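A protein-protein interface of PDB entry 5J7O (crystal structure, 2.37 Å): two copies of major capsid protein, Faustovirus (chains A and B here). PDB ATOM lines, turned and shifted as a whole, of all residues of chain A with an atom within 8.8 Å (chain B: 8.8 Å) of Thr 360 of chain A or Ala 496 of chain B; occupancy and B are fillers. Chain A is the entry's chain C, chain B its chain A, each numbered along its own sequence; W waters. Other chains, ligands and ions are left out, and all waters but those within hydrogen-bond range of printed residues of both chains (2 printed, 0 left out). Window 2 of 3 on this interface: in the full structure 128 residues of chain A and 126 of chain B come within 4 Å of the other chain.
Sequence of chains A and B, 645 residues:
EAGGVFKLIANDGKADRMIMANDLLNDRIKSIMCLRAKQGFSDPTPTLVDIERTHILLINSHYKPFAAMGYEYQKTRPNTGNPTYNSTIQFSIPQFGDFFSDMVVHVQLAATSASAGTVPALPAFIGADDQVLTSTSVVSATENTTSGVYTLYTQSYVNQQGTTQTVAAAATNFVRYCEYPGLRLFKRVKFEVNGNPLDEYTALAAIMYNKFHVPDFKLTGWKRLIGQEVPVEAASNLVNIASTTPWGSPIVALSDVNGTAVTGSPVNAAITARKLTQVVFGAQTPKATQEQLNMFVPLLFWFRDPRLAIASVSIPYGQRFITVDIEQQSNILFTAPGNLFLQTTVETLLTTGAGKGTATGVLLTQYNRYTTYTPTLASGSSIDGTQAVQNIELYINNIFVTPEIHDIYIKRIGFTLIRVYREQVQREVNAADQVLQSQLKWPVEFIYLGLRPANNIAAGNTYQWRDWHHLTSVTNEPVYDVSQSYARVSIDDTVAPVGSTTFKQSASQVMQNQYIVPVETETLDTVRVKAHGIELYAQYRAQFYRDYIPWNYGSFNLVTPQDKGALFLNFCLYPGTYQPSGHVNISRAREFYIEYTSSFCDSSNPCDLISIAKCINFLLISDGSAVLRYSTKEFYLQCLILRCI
The backbone carbonyl oxygen of Tyr 150 of chain A is in hydrogen-bond range of the backbone NH of Leu 349 of chain A, 2.9 Å away. N of Gly 361 of chain A lies close to O of Gly 355 of chain A (3.3 Å). The backbone carbonyl oxygen (O) of Asp 492 of chain B is in hydrogen-bond range of the side-chain hydroxyl (OG) of Ser 490 of chain B. The side-chain hydroxyl of Thr 358 of chain A sits at hydrogen-bond distance from the side-chain hydroxyl of Thr 360 of chain A (3.2 Å).
CG2 of Val 498 of chain B touches CD2 of Leu 349 of chain A (3.97 Å). Phe 503 of chain B touches Leu 349 of chain A (CE2 to CD2, 3.5 Å). Ala 359 of chain A touches Val 498 of chain B. Ala 496 of chain B touches Thr 360 of chain A (CB to O, 3.7 Å). O of Gly 361 of chain A touches CA of Ala 496 of chain B, 3.7 Å away. Gly 361 of chain A touches Pro 497 of chain B. Leu 363 of chain A touches Asp 493 of chain B. Leu 364 of chain A touches Ser 490 of chain B (CB to CB, 3.8 Å). Pro 497 of chain B touches Leu 364 of chain A (CG to CB, 3.6 Å). CE1 of Phe 503 of chain B touches CD2 of Leu 364 of chain A (3.5 Å).
Printed residues of chain B within 4 Å of Ala 359 of chain A: Val 498 (3.4 Å). Of chain B, only Ala 496 (3.7 Å) comes within 4 Å of Thr 360 of chain A. Of chain B, only Ala 496 (3.7 Å) and Pro 497 (3.2 Å) come within 4 Å of Gly 361 of chain A. Printed residues of chain B within 4 Å of Leu 363 of chain A: Asp 493. Printed residues of chain B within 4 Å of Leu 364 of chain A: Ser 490 (3.8 Å), Pro 497 (3.6 Å) and Phe 503 (3.5 Å). Ile 491 of chain B touches none of the printed residues of chain A. Of chain A, only Thr 360 and Gly 361 come within 4 Å of Ala 496 of chain B. Printed residues of chain A within 4 Å of Val 498 of chain B: Leu 349 and Ala 359. Ser 500 of chain B touches none of the printed residues of chain A. Printed residues of chain A within 4 Å of Phe 503 of chain B: Leu 349 and Leu 364. The nearest residue of chain A that does not touch Ala 496 of chain B is Ala 359 of chain A (4.1 Å). The nearest printed residue of chain A that does not touch Asp 493 of chain B is Val 362 of chain A (4.04 Å).
Hydrophobic or aromatic side chains of chain A within 4 Å of the printed part of chain B: Leu 349, Leu 363 and Leu 364. Of the 14 printed residues of chain B, 6 touch a printed residue of chain A. Printed residues of chain B that touch a printed residue of chain A: Ser 490, Asp 493, Ala 496, Pro 497, Val 498 and Phe 503. Among the printed residues, 10 pairs touch across the chains. Among the printed residues, no Asp or Glu carboxylate lies within 4 Å of a Lys or Arg side-chain nitrogen of the other chain.
No position is printed for both chains.
Water W1 lies within hydrogen-bond range of the backbone NH of Leu 363 of chain A, the backbone carbonyl oxygen of Val 495 of chain B and the backbone carbonyl oxygen of Asp 492 of chain B. Water W2 lies within hydrogen-bond range of OG of Ser 490 of chain B (2.6 Å), OD1 of Asp 493 of chain B (2.6 Å), N of Leu 364 of chain A (2.9 Å) and O of Asp 492 of chain B (3.2 Å).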
ATOM      1  N   ASP A 130     -37.672  11.076  25.020  1.00  0.00           N
ATOM      2  CA  ASP A 130     -36.461  11.874  25.217  1.00  0.00           C
ATOM      3  C   ASP A 130     -36.750  13.150  26.007  1.00  0.00           C
ATOM      4  O   ASP A 130     -36.357  14.255  25.624  1.00  0.00           O
ATOM      5  CB  ASP A 130     -35.806  12.197  23.873  1.00  0.00           C
ATOM      6  CG  ASP A 130     -35.629  10.967  23.000  1.00  0.00           C
ATOM      7  OD1 ASP A 130     -35.440   9.863  23.553  1.00  0.00           O
ATOM      8  OD2 ASP A 130     -35.685  11.106  21.760  1.00  0.00           O
ATOM      9  N   GLU A 143     -41.274  10.232  18.289  1.00  0.00           N
ATOM     10  CA  GLU A 143     -40.641   9.410  17.271  1.00  0.00           C
ATOM     11  C   GLU A 143     -41.641   9.027  16.186  1.00  0.00           C
ATOM     12  O   GLU A 143     -42.858   9.072  16.379  1.00  0.00           O
ATOM     13  CB  GLU A 143     -40.038   8.148  17.890  1.00  0.00           C
ATOM     14  CG  GLU A 143     -38.897   8.406  18.859  1.00  0.00           C
ATOM     15  CD  GLU A 143     -38.417   7.137  19.537  1.00  0.00           C
ATOM     16  OE1 GLU A 143     -38.999   6.065  19.269  1.00  0.00           O
ATOM     17  OE2 GLU A 143     -37.462   7.211  20.338  1.00  0.00           O
ATOM     18  N   THR A 145     -40.718   6.074  13.340  1.00  0.00           N
ATOM     19  CA  THR A 145     -39.860   5.236  12.509  1.00  0.00           C
ATOM     20  C   THR A 145     -40.524   4.813  11.207  1.00  0.00           C
ATOM     21  O   THR A 145     -39.823   4.356  10.298  1.00  0.00           O
ATOM     22  CB  THR A 145     -39.425   3.994  13.286  1.00  0.00           C
ATOM     23  OG1 THR A 145     -40.573   3.187  13.582  1.00  0.00           O
ATOM     24  CG2 THR A 145     -38.751   4.399  14.581  1.00  0.00           C
ATOM     25  N   TYR A 150     -38.316  12.806  12.957  1.00  0.00           N
ATOM     26  CA  TYR A 150     -38.093  12.944  14.390  1.00  0.00           C
ATOM     27  C   TYR A 150     -38.443  14.371  14.792  1.00  0.00           C
ATOM     28  O   TYR A 150     -37.800  15.322  14.334  1.00  0.00           O
ATOM     29  CB  TYR A 150     -36.644  12.606  14.743  1.00  0.00           C
ATOM     30  CG  TYR A 150     -36.282  12.740  16.207  1.00  0.00           C
ATOM     31  CD1 TYR A 150     -36.768  11.845  17.151  1.00  0.00           C
ATOM     32  CD2 TYR A 150     -35.428  13.747  16.640  1.00  0.00           C
ATOM     33  CE1 TYR A 150     -36.428  11.961  18.489  1.00  0.00           C
ATOM     34  CE2 TYR A 150     -35.083  13.870  17.972  1.00  0.00           C
ATOM     35  CZ  TYR A 150     -35.584  12.975  18.891  1.00  0.00           C
ATOM     36  OH  TYR A 150     -35.239  13.098  20.219  1.00  0.00           O
ATOM     37  N   LEU A 349     -36.677  16.457  11.927  1.00  0.00           N
ATOM     38  CA  LEU A 349     -35.504  15.946  11.227  1.00  0.00           C
ATOM     39  C   LEU A 349     -35.911  14.699  10.457  1.00  0.00           C
ATOM     40  O   LEU A 349     -36.325  13.703  11.061  1.00  0.00           O
ATOM     41  CB  LEU A 349     -34.367  15.623  12.200  1.00  0.00           C
ATOM     42  CG  LEU A 349     -33.658  16.755  12.947  1.00  0.00           C
ATOM     43  CD1 LEU A 349     -34.473  17.237  14.138  1.00  0.00           C
ATOM     44  CD2 LEU A 349     -32.279  16.294  13.391  1.00  0.00           C
ATOM     45  N   THR A 351     -34.700  11.694   8.485  1.00  0.00           N
ATOM     46  CA  THR A 351     -33.615  10.791   8.140  1.00  0.00           C
ATOM     47  C   THR A 351     -34.171   9.583   7.395  1.00  0.00           C
ATOM     48  O   THR A 351     -35.352   9.244   7.510  1.00  0.00           O
ATOM     49  CB  THR A 351     -32.851  10.336   9.388  1.00  0.00           C
ATOM     50  OG1 THR A 351     -33.766   9.771  10.334  1.00  0.00           O
ATOM     51  CG2 THR A 351     -32.120  11.510  10.026  1.00  0.00           C
ATOM     52  N   GLY A 353     -31.963   6.532   6.927  1.00  0.00           N
ATOM     53  CA  GLY A 353     -31.161   5.363   7.205  1.00  0.00           C
ATOM     54  C   GLY A 353     -31.640   4.593   8.418  1.00  0.00           C
ATOM     55  O   GLY A 353     -32.803   4.680   8.830  1.00  0.00           O
ATOM     56  N   ALA A 354     -30.723   3.820   8.997  1.00  0.00           N
ATOM     57  CA  ALA A 354     -31.050   3.015  10.166  1.00  0.00           C
ATOM     58  C   ALA A 354     -31.399   3.907  11.350  1.00  0.00           C
ATOM     59  O   ALA A 354     -30.730   4.910  11.615  1.00  0.00           O
ATOM     60  CB  ALA A 354     -29.879   2.099  10.521  1.00  0.00           C
ATOM     61  N   GLY A 355     -32.459   3.534  12.062  1.00  0.00           N
ATOM     62  CA  GLY A 355     -32.935   4.322  13.179  1.00  0.00           C
ATOM     63  C   GLY A 355     -33.723   5.553  12.799  1.00  0.00           C
ATOM     64  O   GLY A 355     -33.927   6.422  13.655  1.00  0.00           O
ATOM     65  N   LYS A 356     -34.170   5.655  11.548  1.00  0.00           N
ATOM     66  CA  LYS A 356     -34.912   6.825  11.098  1.00  0.00           C
ATOM     67  C   LYS A 356     -36.139   7.057  11.973  1.00  0.00           C
ATOM     68  O   LYS A 356     -36.775   6.115  12.453  1.00  0.00           O
ATOM     69  CB  LYS A 356     -35.331   6.661   9.636  1.00  0.00           C
ATOM     70  CG  LYS A 356     -36.195   5.441   9.364  1.00  0.00           C
ATOM     71  CD  LYS A 356     -36.668   5.405   7.919  1.00  0.00           C
ATOM     72  CE  LYS A 356     -37.619   4.242   7.679  1.00  0.00           C
ATOM     73  NZ  LYS A 356     -38.187   4.267   6.302  1.00  0.00           N
ATOM     74  N   GLY A 357     -36.461   8.332  12.185  1.00  0.00           N
ATOM     75  CA  GLY A 357     -37.555   8.712  13.049  1.00  0.00           C
ATOM     76  C   GLY A 357     -37.201   8.814  14.516  1.00  0.00           C
ATOM     77  O   GLY A 357     -38.033   9.282  15.302  1.00  0.00           O
ATOM     78  N   THR A 358     -36.007   8.386  14.910  1.00  0.00           N
ATOM     79  CA  THR A 358     -35.525   8.502  16.279  1.00  0.00           C
ATOM     80  C   THR A 358     -34.313   9.427  16.312  1.00  0.00           C
ATOM     81  O   THR A 358     -33.832   9.900  15.280  1.00  0.00           O
ATOM     82  CB  THR A 358     -35.164   7.131  16.861  1.00  0.00           C
ATOM     83  OG1 THR A 358     -33.897   6.707  16.344  1.00  0.00           O
ATOM     84  CG2 THR A 358     -36.217   6.104  16.495  1.00  0.00           C
ATOM     85  N   ALA A 359     -33.815   9.677  17.525  1.00  0.00           N
ATOM     86  CA  ALA A 359     -32.679  10.574  17.690  1.00  0.00           C
ATOM     87  C   ALA A 359     -31.390   9.986  17.135  1.00  0.00           C
ATOM     88  O   ALA A 359     -30.414  10.723  16.960  1.00  0.00           O
ATOM     89  CB  ALA A 359     -32.496  10.928  19.166  1.00  0.00           C
ATOM     90  N   THR A 360     -31.362   8.686  16.853  1.00  0.00           N
ATOM     91  CA  THR A 360     -30.169   8.031  16.341  1.00  0.00           C
ATOM     92  C   THR A 360     -30.263   7.711  14.855  1.00  0.00           C
ATOM     93  O   THR A 360     -29.432   6.956  14.344  1.00  0.00           O
ATOM     94  CB  THR A 360     -29.884   6.750  17.130  1.00  0.00           C
ATOM     95  OG1 THR A 360     -30.931   5.798  16.904  1.00  0.00           O
ATOM     96  CG2 THR A 360     -29.786   7.049  18.619  1.00  0.00           C
ATOM     97  N   GLY A 361     -31.249   8.264  14.152  1.00  0.00           N
ATOM     98  CA  GLY A 361     -31.351   8.027  12.723  1.00  0.00           C
ATOM     99  C   GLY A 361     -30.266   8.768  11.958  1.00  0.00           C
ATOM    100  O   GLY A 361     -29.876   9.880  12.313  1.00  0.00           O
ATOM    101  N   VAL A 362     -29.781   8.139  10.892  1.00  0.00           N
ATOM    102  CA  VAL A 362     -28.657   8.659  10.129  1.00  0.00           C
ATOM    103  C   VAL A 362     -29.147   9.157   8.772  1.00  0.00           C
ATOM    104  O   VAL A 362     -30.257   8.857   8.334  1.00  0.00           O
ATOM    105  CB  VAL A 362     -27.539   7.609   9.962  1.00  0.00           C
ATOM    106  CG1 VAL A 362     -27.156   7.023  11.315  1.00  0.00           C
ATOM    107  CG2 VAL A 362     -27.978   6.514   8.998  1.00  0.00           C
ATOM    108  N   LEU A 363     -28.288   9.931   8.102  1.00  0.00           N
ATOM    109  CA  LEU A 363     -28.559  10.518   6.793  1.00  0.00           C
ATOM    110  C   LEU A 363     -29.730  11.492   6.865  1.00  0.00           C
ATOM    111  O   LEU A 363     -30.868  11.130   6.551  1.00  0.00           O
ATOM    112  CB  LEU A 363     -28.823   9.426   5.748  1.00  0.00           C
ATOM    113  CG  LEU A 363     -28.941   9.847   4.278  1.00  0.00           C
ATOM    114  CD1 LEU A 363     -28.401   8.752   3.370  1.00  0.00           C
ATOM    115  CD2 LEU A 363     -30.376  10.191   3.903  1.00  0.00           C
ATOM    116  N   LEU A 364     -29.454  12.732   7.264  1.00  0.00           N
ATOM    117  CA  LEU A 364     -30.482  13.756   7.406  1.00  0.00           C
ATOM    118  C   LEU A 364     -30.668  14.484   6.080  1.00  0.00           C
ATOM    119  O   LEU A 364     -29.744  15.146   5.596  1.00  0.00           O
ATOM    120  CB  LEU A 364     -30.110  14.747   8.506  1.00  0.00           C
ATOM    121  CG  LEU A 364     -31.046  15.951   8.608  1.00  0.00           C
ATOM    122  CD1 LEU A 364     -32.431  15.514   9.059  1.00  0.00           C
ATOM    123  CD2 LEU A 364     -30.482  17.004   9.543  1.00  0.00           C
ATOM    124  N   SER B 490     -26.692  18.513   8.258  1.00  0.00           N
ATOM    125  CA  SER B 490     -25.794  17.403   8.545  1.00  0.00           C
ATOM    126  C   SER B 490     -24.757  17.298   7.434  1.00  0.00           C
ATOM    127  O   SER B 490     -25.111  17.227   6.252  1.00  0.00           O
ATOM    128  CB  SER B 490     -26.573  16.092   8.666  1.00  0.00           C
ATOM    129  OG  SER B 490     -25.701  14.976   8.636  1.00  0.00           O
ATOM    130  N   ILE B 491     -23.479  17.291   7.811  1.00  0.00           N
ATOM    131  CA  ILE B 491     -22.389  17.245   6.845  1.00  0.00           C
ATOM    132  C   ILE B 491     -21.729  15.872   6.796  1.00  0.00           C
ATOM    133  O   ILE B 491     -20.715  15.701   6.110  1.00  0.00           O
ATOM    134  CB  ILE B 491     -21.347  18.342   7.119  1.00  0.00           C
ATOM    135  CG1 ILE B 491     -20.532  18.011   8.371  1.00  0.00           C
ATOM    136  CG2 ILE B 491     -22.028  19.696   7.266  1.00  0.00           C
ATOM    137  CD1 ILE B 491     -19.249  18.805   8.483  1.00  0.00           C
ATOM    138  N   ASP B 492     -22.275  14.888   7.507  1.00  0.00           N
ATOM    139  CA  ASP B 492     -21.788  13.513   7.442  1.00  0.00           C
ATOM    140  C   ASP B 492     -22.990  12.583   7.458  1.00  0.00           C
ATOM    141  O   ASP B 492     -23.734  12.550   8.442  1.00  0.00           O
ATOM    142  CB  ASP B 492     -20.842  13.194   8.605  1.00  0.00           C
ATOM    143  CG  ASP B 492     -20.125  11.862   8.430  1.00  0.00           C
ATOM    144  OD1 ASP B 492     -20.510  11.079   7.536  1.00  0.00           O
ATOM    145  OD2 ASP B 492     -19.173  11.593   9.192  1.00  0.00           O
ATOM    146  N   ASP B 493     -23.169  11.825   6.378  1.00  0.00           N
ATOM    147  CA  ASP B 493     -24.319  10.940   6.243  1.00  0.00           C
ATOM    148  C   ASP B 493     -24.179   9.639   7.023  1.00  0.00           C
ATOM    149  O   ASP B 493     -25.099   8.814   6.978  1.00  0.00           O
ATOM    150  CB  ASP B 493     -24.572  10.626   4.766  1.00  0.00           C
ATOM    151  CG  ASP B 493     -25.241  11.773   4.033  1.00  0.00           C
ATOM    152  OD1 ASP B 493     -25.909  12.596   4.695  1.00  0.00           O
ATOM    153  OD2 ASP B 493     -25.107  11.848   2.793  1.00  0.00           O
ATOM    154  N   THR B 494     -23.073   9.427   7.736  1.00  0.00           N
ATOM    155  CA  THR B 494     -22.890   8.217   8.527  1.00  0.00           C
ATOM    156  C   THR B 494     -22.946   8.468  10.027  1.00  0.00           C
ATOM    157  O   THR B 494     -22.861   7.511  10.804  1.00  0.00           O
ATOM    158  CB  THR B 494     -21.560   7.539   8.173  1.00  0.00           C
ATOM    159  OG1 THR B 494     -20.477   8.254   8.779  1.00  0.00           O
ATOM    160  CG2 THR B 494     -21.360   7.509   6.663  1.00  0.00           C
ATOM    161  N   VAL B 495     -23.086   9.720  10.458  1.00  0.00           N
ATOM    162  CA  VAL B 495     -23.169  10.071  11.871  1.00  0.00           C
ATOM    163  C   VAL B 495     -24.562  10.620  12.146  1.00  0.00           C
ATOM    164  O   VAL B 495     -25.064  11.461  11.392  1.00  0.00           O
ATOM    165  CB  VAL B 495     -22.086  11.090  12.266  1.00  0.00           C
ATOM    166  CG1 VAL B 495     -22.112  11.341  13.767  1.00  0.00           C
ATOM    167  CG2 VAL B 495     -20.716  10.602  11.829  1.00  0.00           C
ATOM    168  N   ALA B 496     -25.182  10.143  13.222  1.00  0.00           N
ATOM    169  CA  ALA B 496     -26.512  10.616  13.588  1.00  0.00           C
ATOM    170  C   ALA B 496     -26.450  12.092  13.967  1.00  0.00           C
ATOM    171  O   ALA B 496     -25.620  12.478  14.799  1.00  0.00           O
ATOM    172  CB  ALA B 496     -27.075   9.790  14.741  1.00  0.00           C
ATOM    173  N   PRO B 497     -27.301  12.942  13.387  1.00  0.00           N
ATOM    174  CA  PRO B 497     -27.156  14.392  13.611  1.00  0.00           C
ATOM    175  C   PRO B 497     -27.379  14.830  15.050  1.00  0.00           C
ATOM    176  O   PRO B 497     -26.655  15.707  15.536  1.00  0.00           O
ATOM    177  CB  PRO B 497     -28.211  14.994  12.671  1.00  0.00           C
ATOM    178  CG  PRO B 497     -28.463  13.940  11.644  1.00  0.00           C
ATOM    179  CD  PRO B 497     -28.312  12.637  12.361  1.00  0.00           C
ATOM    180  N   VAL B 498     -28.361  14.251  15.743  1.00  0.00           N
ATOM    181  CA  VAL B 498     -28.743  14.749  17.062  1.00  0.00           C
ATOM    182  C   VAL B 498     -27.580  14.587  18.030  1.00  0.00           C
ATOM    183  O   VAL B 498     -27.081  13.475  18.248  1.00  0.00           O
ATOM    184  CB  VAL B 498     -29.998  14.032  17.569  1.00  0.00           C
ATOM    185  CG1 VAL B 498     -30.317  14.469  18.990  1.00  0.00           C
ATOM    186  CG2 VAL B 498     -31.173  14.312  16.645  1.00  0.00           C
ATOM    187  N   GLY B 499     -27.142  15.699  18.616  1.00  0.00           N
ATOM    188  CA  GLY B 499     -26.060  15.666  19.580  1.00  0.00           C
ATOM    189  C   GLY B 499     -24.679  15.534  18.985  1.00  0.00           C
ATOM    190  O   GLY B 499     -23.776  15.011  19.646  1.00  0.00           O
ATOM    191  N   SER B 500     -24.481  15.999  17.755  1.00  0.00           N
ATOM    192  CA  SER B 500     -23.209  15.861  17.062  1.00  0.00           C
ATOM    193  C   SER B 500     -22.746  17.216  16.547  1.00  0.00           C
ATOM    194  O   SER B 500     -23.558  18.081  16.209  1.00  0.00           O
ATOM    195  CB  SER B 500     -23.317  14.870  15.893  1.00  0.00           C
ATOM    196  OG  SER B 500     -22.100  14.794  15.170  1.00  0.00           O
ATOM    197  N   THR B 501     -21.425  17.394  16.496  1.00  0.00           N
ATOM    198  CA  THR B 501     -20.850  18.600  15.913  1.00  0.00           C
ATOM    199  C   THR B 501     -20.898  18.598  14.392  1.00  0.00           C
ATOM    200  O   THR B 501     -20.606  19.631  13.779  1.00  0.00           O
ATOM    201  CB  THR B 501     -19.403  18.786  16.381  1.00  0.00           C
ATOM    202  OG1 THR B 501     -18.690  17.551  16.245  1.00  0.00           O
ATOM    203  CG2 THR B 501     -19.365  19.240  17.835  1.00  0.00           C
ATOM    204  N   THR B 502     -21.248  17.472  13.770  1.00  0.00           N
ATOM    205  CA  THR B 502     -21.519  17.434  12.339  1.00  0.00           C
ATOM    206  C   THR B 502     -22.893  17.994  11.996  1.00  0.00           C
ATOM    207  O   THR B 502     -23.228  18.090  10.809  1.00  0.00           O
ATOM    208  CB  THR B 502     -21.400  15.999  11.814  1.00  0.00           C
ATOM    209  OG1 THR B 502     -22.311  15.150  12.524  1.00  0.00           O
ATOM    210  CG2 THR B 502     -19.983  15.478  11.999  1.00  0.00           C
ATOM    211  N   PHE B 503     -23.686  18.359  13.002  1.00  0.00           N
ATOM    212  CA  PHE B 503     -25.005  18.960  12.820  1.00  0.00           C
ATOM    213  C   PHE B 503     -24.830  20.469  12.975  1.00  0.00           C
ATOM    214  O   PHE B 503     -24.849  21.006  14.082  1.00  0.00           O
ATOM    215  CB  PHE B 503     -25.994  18.390  13.831  1.00  0.00           C
ATOM    216  CG  PHE B 503     -27.433  18.617  13.472  1.00  0.00           C
ATOM    217  CD1 PHE B 503     -27.794  18.996  12.192  1.00  0.00           C
ATOM    218  CD2 PHE B 503     -28.426  18.460  14.425  1.00  0.00           C
ATOM    219  CE1 PHE B 503     -29.115  19.208  11.866  1.00  0.00           C
ATOM    220  CE2 PHE B 503     -29.750  18.674  14.106  1.00  0.00           C
ATOM    221  CZ  PHE B 503     -30.096  19.049  12.825  1.00  0.00           C
HETATM  222  O   HOH W   1     -26.743  11.193   9.446  1.00  0.00           O
HETATM  223  O   HOH W   2     -26.610  13.021   7.183  1.00  0.00           O
